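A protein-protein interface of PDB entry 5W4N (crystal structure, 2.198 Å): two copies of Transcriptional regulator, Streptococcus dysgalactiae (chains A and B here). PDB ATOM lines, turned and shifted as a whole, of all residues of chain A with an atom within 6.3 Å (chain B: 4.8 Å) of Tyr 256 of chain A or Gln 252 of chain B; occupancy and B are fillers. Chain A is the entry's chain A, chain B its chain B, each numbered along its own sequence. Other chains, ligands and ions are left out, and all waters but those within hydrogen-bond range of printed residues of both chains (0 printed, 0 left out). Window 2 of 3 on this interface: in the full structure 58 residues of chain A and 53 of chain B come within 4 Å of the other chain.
The side-chain amide nitrogen of Gln 252 of chain A is in hydrogen-bond range of the side-chain hydroxyl of Tyr 256 of chain B, 3.1 Å away.
OE1 of Gln 252 of chain B sits at hydrogen-bond distance from OH of Tyr 256 of chain A.
The side-chain hydroxyl (OH) of Tyr 256 of chain A sits at hydrogen-bond distance from the side-chain amide nitrogen (NE2) of Gln 252 of chain A (3.3 Å).
The side-chain amide oxygen of Gln 252 of chain B sits at hydrogen-bond distance from the side-chain hydroxyl of Tyr 256 of chain B, 3.2 Å away.
OE1 of Gln 252 of chain B touches NE2 of Gln 252 of chain A, 3.7 Å away.
Leu 228 of chain B touches Tyr 256 of chain A.
Gln 249 of chain B touches Tyr 256 of chain A (CD to CD1, 3.5 Å).
Leu 257 of chain A touches Ile 253 of chain B (CD2 to CD1, 3.8 Å).
Of the printed residues of chain B, Gln 252 of chain A touches Gln 252 and Tyr 256.
Lys 255 of chain A touches none of the printed residues of chain B.
Of chain B, only Leu 228, Gln 249 and Gln 252 come within 4 Å of Tyr 256 of chain A.
Printed residues of chain B within 4 Å of Leu 257 of chain A: Ile 253.
Printed residues of chain A within 4 Å of Leu 228 of chain B: Tyr 256.
Arg 248 of chain B touches none of the printed residues of chain A.
Of the printed residues of chain A, Gln 249 of chain B touches Tyr 256 (3.5 Å).
Of chain A, only Gln 252 and Tyr 256 come within 4 Å of Gln 252 of chain B.
Printed residues of chain A within 4 Å of Tyr 256 of chain B: Gln 252.
The nearest residue of chain B that does not touch Tyr 256 of chain A is Ile 253 of chain B (4.1 Å).
Hydrophobic or aromatic side chains of chain B within 4 Å of the printed part of chain A: Leu 228, Ile 253 and Tyr 256.
Of the 9 printed residues of chain A, 3 touch a printed residue of chain B.
Hydrophobic or aromatic side chains of chain A that line the printed part of chain B: Tyr 256 and Leu 257.
Gln 252 of chain B touches its own counterpart, Gln 252 of chain A.
Gln 252 of chain A touches Tyr 256 of chain B, and with the chains exchanged Tyr 256 of chain A touches Gln 252 of chain B.
6 positions are printed for both chains.
Of the 6 pairs that touch across the chains among the printed residues, 3 have their exchanged pair printed and touching as well.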
ATOM      1  N   LEU A 251     -23.614 -22.534  16.276  1.00  0.00           N
ATOM      2  CA  LEU A 251     -23.916 -23.800  15.617  1.00  0.00           C
ATOM      3  C   LEU A 251     -24.515 -24.800  16.598  1.00  0.00           C
ATOM      4  O   LEU A 251     -25.423 -25.562  16.243  1.00  0.00           O
ATOM      5  CB  LEU A 251     -22.651 -24.367  14.975  1.00  0.00           C
ATOM      6  CG  LEU A 251     -22.190 -23.646  13.710  1.00  0.00           C
ATOM      7  CD1 LEU A 251     -20.708 -23.880  13.463  1.00  0.00           C
ATOM      8  CD2 LEU A 251     -23.019 -24.103  12.525  1.00  0.00           C
ATOM      9  N   GLN A 252     -24.022 -24.811  17.839  1.00  0.00           N
ATOM     10  CA  GLN A 252     -24.581 -25.704  18.848  1.00  0.00           C
ATOM     11  C   GLN A 252     -26.014 -25.318  19.193  1.00  0.00           C
ATOM     12  O   GLN A 252     -26.846 -26.188  19.482  1.00  0.00           O
ATOM     13  CB  GLN A 252     -23.706 -25.696  20.101  1.00  0.00           C
ATOM     14  CG  GLN A 252     -22.575 -26.709  20.067  1.00  0.00           C
ATOM     15  CD  GLN A 252     -21.654 -26.594  21.265  1.00  0.00           C
ATOM     16  OE1 GLN A 252     -20.468 -26.910  21.181  1.00  0.00           O
ATOM     17  NE2 GLN A 252     -22.197 -26.139  22.388  1.00  0.00           N
ATOM     18  N   ILE A 253     -26.320 -24.019  19.177  1.00  0.00           N
ATOM     19  CA  ILE A 253     -27.693 -23.579  19.410  1.00  0.00           C
ATOM     20  C   ILE A 253     -28.611 -24.123  18.322  1.00  0.00           C
ATOM     21  O   ILE A 253     -29.689 -24.659  18.603  1.00  0.00           O
ATOM     22  CB  ILE A 253     -27.764 -22.043  19.491  1.00  0.00           C
ATOM     23  CG1 ILE A 253     -26.983 -21.532  20.701  1.00  0.00           C
ATOM     24  CG2 ILE A 253     -29.213 -21.576  19.556  1.00  0.00           C
ATOM     25  CD1 ILE A 253     -26.928 -20.024  20.792  1.00  0.00           C
ATOM     26  N   PHE A 254     -28.191 -23.990  17.060  1.00  0.00           N
ATOM     27  CA  PHE A 254     -28.960 -24.557  15.956  1.00  0.00           C
ATOM     28  C   PHE A 254     -29.149 -26.058  16.131  1.00  0.00           C
ATOM     29  O   PHE A 254     -30.250 -26.582  15.922  1.00  0.00           O
ATOM     30  CB  PHE A 254     -28.265 -24.270  14.623  1.00  0.00           C
ATOM     31  CG  PHE A 254     -28.337 -22.833  14.190  1.00  0.00           C
ATOM     32  CD1 PHE A 254     -29.478 -22.080  14.413  1.00  0.00           C
ATOM     33  CD2 PHE A 254     -27.264 -22.239  13.544  1.00  0.00           C
ATOM     34  CE1 PHE A 254     -29.545 -20.758  14.008  1.00  0.00           C
ATOM     35  CE2 PHE A 254     -27.323 -20.918  13.138  1.00  0.00           C
ATOM     36  CZ  PHE A 254     -28.465 -20.176  13.370  1.00  0.00           C
ATOM     37  N   LYS A 255     -28.086 -26.766  16.519  1.00  0.00           N
ATOM     38  CA  LYS A 255     -28.172 -28.216  16.655  1.00  0.00           C
ATOM     39  C   LYS A 255     -29.089 -28.618  17.804  1.00  0.00           C
ATOM     40  O   LYS A 255     -29.885 -29.554  17.671  1.00  0.00           O
ATOM     41  CB  LYS A 255     -26.777 -28.811  16.848  1.00  0.00           C
ATOM     42  CG  LYS A 255     -26.773 -30.324  17.006  1.00  0.00           C
ATOM     43  CD  LYS A 255     -25.444 -30.932  16.580  1.00  0.00           C
ATOM     44  CE  LYS A 255     -24.289 -30.380  17.400  1.00  0.00           C
ATOM     45  NZ  LYS A 255     -24.360 -30.818  18.821  1.00  0.00           N
ATOM     46  N   TYR A 256     -28.994 -27.922  18.941  1.00  0.00           N
ATOM     47  CA  TYR A 256     -29.819 -28.275  20.092  1.00  0.00           C
ATOM     48  C   TYR A 256     -31.299 -28.028  19.828  1.00  0.00           C
ATOM     49  O   TYR A 256     -32.150 -28.744  20.365  1.00  0.00           O
ATOM     50  CB  TYR A 256     -29.375 -27.490  21.328  1.00  0.00           C
ATOM     51  CG  TYR A 256     -27.977 -27.810  21.811  1.00  0.00           C
ATOM     52  CD1 TYR A 256     -27.344 -28.993  21.448  1.00  0.00           C
ATOM     53  CD2 TYR A 256     -27.292 -26.928  22.636  1.00  0.00           C
ATOM     54  CE1 TYR A 256     -26.065 -29.284  21.892  1.00  0.00           C
ATOM     55  CE2 TYR A 256     -26.016 -27.210  23.084  1.00  0.00           C
ATOM     56  CZ  TYR A 256     -25.408 -28.389  22.710  1.00  0.00           C
ATOM     57  OH  TYR A 256     -24.135 -28.668  23.157  1.00  0.00           O
ATOM     58  N   LEU A 257     -31.625 -27.027  19.015  1.00  0.00           N
ATOM     59  CA  LEU A 257     -33.011 -26.685  18.727  1.00  0.00           C
ATOM     60  C   LEU A 257     -33.592 -27.470  17.559  1.00  0.00           C
ATOM     61  O   LEU A 257     -34.747 -27.237  17.189  1.00  0.00           O
ATOM     62  CB  LEU A 257     -33.135 -25.183  18.452  1.00  0.00           C
ATOM     63  CG  LEU A 257     -32.875 -24.278  19.659  1.00  0.00           C
ATOM     64  CD1 LEU A 257     -32.976 -22.812  19.269  1.00  0.00           C
ATOM     65  CD2 LEU A 257     -33.838 -24.607  20.790  1.00  0.00           C
ATOM     66  N   GLY A 258     -32.829 -28.391  16.975  1.00  0.00           N
ATOM     67  CA  GLY A 258     -33.328 -29.151  15.847  1.00  0.00           C
ATOM     68  C   GLY A 258     -33.456 -28.367  14.563  1.00  0.00           C
ATOM     69  O   GLY A 258     -34.217 -28.766  13.678  1.00  0.00           O
ATOM     70  N   GLU A 259     -32.734 -27.253  14.437  1.00  0.00           N
ATOM     71  CA  GLU A 259     -32.774 -26.424  13.232  1.00  0.00           C
ATOM     72  C   GLU A 259     -31.726 -26.951  12.255  1.00  0.00           C
ATOM     73  O   GLU A 259     -30.633 -26.401  12.102  1.00  0.00           O
ATOM     74  CB  GLU A 259     -32.544 -24.960  13.580  1.00  0.00           C
ATOM     75  CG  GLU A 259     -33.577 -24.383  14.533  1.00  0.00           C
ATOM     76  CD  GLU A 259     -34.925 -24.184  13.872  1.00  0.00           C
ATOM     77  OE1 GLU A 259     -34.959 -23.989  12.638  1.00  0.00           O
ATOM     78  OE2 GLU A 259     -35.950 -24.221  14.584  1.00  0.00           O
ATOM     79  N   LEU B 228     -37.565 -26.848  24.930  1.00  0.00           N
ATOM     80  CA  LEU B 228     -36.532 -27.871  25.067  1.00  0.00           C
ATOM     81  C   LEU B 228     -36.297 -28.218  26.531  1.00  0.00           C
ATOM     82  O   LEU B 228     -36.183 -29.396  26.890  1.00  0.00           O
ATOM     83  CB  LEU B 228     -35.234 -27.395  24.411  1.00  0.00           C
ATOM     84  CG  LEU B 228     -34.017 -28.318  24.512  1.00  0.00           C
ATOM     85  CD1 LEU B 228     -34.269 -29.626  23.780  1.00  0.00           C
ATOM     86  CD2 LEU B 228     -32.772 -27.634  23.969  1.00  0.00           C
ATOM     87  N   ARG B 248     -29.934 -29.456  29.976  1.00  0.00           N
ATOM     88  CA  ARG B 248     -28.598 -28.869  29.995  1.00  0.00           C
ATOM     89  C   ARG B 248     -28.320 -28.090  28.715  1.00  0.00           C
ATOM     90  O   ARG B 248     -27.666 -27.041  28.750  1.00  0.00           O
ATOM     91  CB  ARG B 248     -27.546 -29.960  30.203  1.00  0.00           C
ATOM     92  CG  ARG B 248     -27.552 -30.564  31.601  1.00  0.00           C
ATOM     93  CD  ARG B 248     -26.268 -31.328  31.880  1.00  0.00           C
ATOM     94  NE  ARG B 248     -26.359 -32.728  31.475  1.00  0.00           N
ATOM     95  CZ  ARG B 248     -26.313 -33.754  32.319  1.00  0.00           C
ATOM     96  NH1 ARG B 248     -26.176 -33.540  33.620  1.00  0.00           N
ATOM     97  NH2 ARG B 248     -26.403 -34.996  31.861  1.00  0.00           N
ATOM     98  N   GLN B 249     -28.809 -28.587  27.577  1.00  0.00           N
ATOM     99  CA  GLN B 249     -28.635 -27.862  26.322  1.00  0.00           C
ATOM    100  C   GLN B 249     -29.383 -26.536  26.345  1.00  0.00           C
ATOM    101  O   GLN B 249     -28.893 -25.529  25.820  1.00  0.00           O
ATOM    102  CB  GLN B 249     -29.102 -28.721  25.147  1.00  0.00           C
ATOM    103  CG  GLN B 249     -28.239 -29.944  24.893  1.00  0.00           C
ATOM    104  CD  GLN B 249     -28.870 -30.910  23.910  1.00  0.00           C
ATOM    105  OE1 GLN B 249     -29.990 -30.699  23.444  1.00  0.00           O
ATOM    106  NE2 GLN B 249     -28.154 -31.983  23.596  1.00  0.00           N
ATOM    107  N   ALA B 250     -30.572 -26.515  26.951  1.00  0.00           N
ATOM    108  CA  ALA B 250     -31.322 -25.268  27.066  1.00  0.00           C
ATOM    109  C   ALA B 250     -30.584 -24.261  27.935  1.00  0.00           C
ATOM    110  O   ALA B 250     -30.617 -23.054  27.665  1.00  0.00           O
ATOM    111  CB  ALA B 250     -32.717 -25.546  27.626  1.00  0.00           C
ATOM    112  N   LEU B 251     -29.909 -24.738  28.984  1.00  0.00           N
ATOM    113  CA  LEU B 251     -29.104 -23.848  29.815  1.00  0.00           C
ATOM    114  C   LEU B 251     -27.928 -23.278  29.032  1.00  0.00           C
ATOM    115  O   LEU B 251     -27.582 -22.101  29.190  1.00  0.00           O
ATOM    116  CB  LEU B 251     -28.607 -24.589  31.057  1.00  0.00           C
ATOM    117  CG  LEU B 251     -29.664 -25.093  32.040  1.00  0.00           C
ATOM    118  CD1 LEU B 251     -29.010 -25.852  33.188  1.00  0.00           C
ATOM    119  CD2 LEU B 251     -30.502 -23.939  32.562  1.00  0.00           C
ATOM    120  N   GLN B 252     -27.301 -24.098  28.184  1.00  0.00           N
ATOM    121  CA  GLN B 252     -26.178 -23.617  27.386  1.00  0.00           C
ATOM    122  C   GLN B 252     -26.623 -22.549  26.394  1.00  0.00           C
ATOM    123  O   GLN B 252     -25.871 -21.611  26.102  1.00  0.00           O
ATOM    124  CB  GLN B 252     -25.513 -24.785  26.657  1.00  0.00           C
ATOM    125  CG  GLN B 252     -24.863 -25.805  27.579  1.00  0.00           C
ATOM    126  CD  GLN B 252     -24.279 -26.986  26.826  1.00  0.00           C
ATOM    127  OE1 GLN B 252     -23.764 -26.839  25.716  1.00  0.00           O
ATOM    128  NE2 GLN B 252     -24.358 -28.166  27.428  1.00  0.00           N
ATOM    129  N   ILE B 253     -27.844 -22.673  25.866  1.00  0.00           N
ATOM    130  CA  ILE B 253     -28.360 -21.670  24.935  1.00  0.00           C
ATOM    131  C   ILE B 253     -28.490 -20.320  25.630  1.00  0.00           C
ATOM    132  O   ILE B 253     -28.062 -19.287  25.103  1.00  0.00           O
ATOM    133  CB  ILE B 253     -29.705 -22.126  24.337  1.00  0.00           C
ATOM    134  CG1 ILE B 253     -29.526 -23.411  23.531  1.00  0.00           C
ATOM    135  CG2 ILE B 253     -30.296 -21.031  23.461  1.00  0.00           C
ATOM    136  CD1 ILE B 253     -30.816 -23.955  22.953  1.00  0.00           C
ATOM    137  N   PHE B 254     -29.091 -20.310  26.824  1.00  0.00           N
ATOM    138  CA  PHE B 254     -29.172 -19.078  27.604  1.00  0.00           C
ATOM    139  C   PHE B 254     -27.785 -18.519  27.888  1.00  0.00           C
ATOM    140  O   PHE B 254     -27.577 -17.301  27.863  1.00  0.00           O
ATOM    141  CB  PHE B 254     -29.916 -19.333  28.916  1.00  0.00           C
ATOM    142  CG  PHE B 254     -31.378 -19.638  28.744  1.00  0.00           C
ATOM    143  CD1 PHE B 254     -32.118 -19.024  27.747  1.00  0.00           C
ATOM    144  CD2 PHE B 254     -32.015 -20.532  29.591  1.00  0.00           C
ATOM    145  CE1 PHE B 254     -33.464 -19.302  27.593  1.00  0.00           C
ATOM    146  CE2 PHE B 254     -33.362 -20.815  29.441  1.00  0.00           C
ATOM    147  CZ  PHE B 254     -34.087 -20.199  28.440  1.00  0.00           C
ATOM    148  N   LYS B 255     -26.821 -19.401  28.155  1.00  0.00           N
ATOM    149  CA  LYS B 255     -25.469 -18.963  28.485  1.00  0.00           C
ATOM    150  C   LYS B 255     -24.764 -18.379  27.265  1.00  0.00           C
ATOM    151  O   LYS B 255     -24.149 -17.309  27.345  1.00  0.00           O
ATOM    152  CB  LYS B 255     -24.683 -20.140  29.066  1.00  0.00           C
ATOM    153  CG  LYS B 255     -23.198 -19.897  29.272  1.00  0.00           C
ATOM    154  CD  LYS B 255     -22.513 -21.185  29.714  1.00  0.00           C
ATOM    155  CE  LYS B 255     -21.002 -21.107  29.572  1.00  0.00           C
ATOM    156  NZ  LYS B 255     -20.384 -20.262  30.630  1.00  0.00           N
ATOM    157  N   TYR B 256     -24.853 -19.063  26.121  1.00  0.00           N
ATOM    158  CA  TYR B 256     -24.152 -18.605  24.925  1.00  0.00           C
ATOM    159  C   TYR B 256     -24.700 -17.277  24.417  1.00  0.00           C
ATOM    160  O   TYR B 256     -23.958 -16.490  23.818  1.00  0.00           O
ATOM    161  CB  TYR B 256     -24.242 -19.660  23.822  1.00  0.00           C
ATOM    162  CG  TYR B 256     -23.537 -20.961  24.135  1.00  0.00           C
ATOM    163  CD1 TYR B 256     -22.550 -21.025  25.111  1.00  0.00           C
ATOM    164  CD2 TYR B 256     -23.856 -22.125  23.451  1.00  0.00           C
ATOM    165  CE1 TYR B 256     -21.903 -22.213  25.396  1.00  0.00           C
ATOM    166  CE2 TYR B 256     -23.217 -23.317  23.728  1.00  0.00           C
ATOM    167  CZ  TYR B 256     -22.241 -23.355  24.700  1.00  0.00           C
ATOM    168  OH  TYR B 256     -21.603 -24.541  24.979  1.00  0.00           O
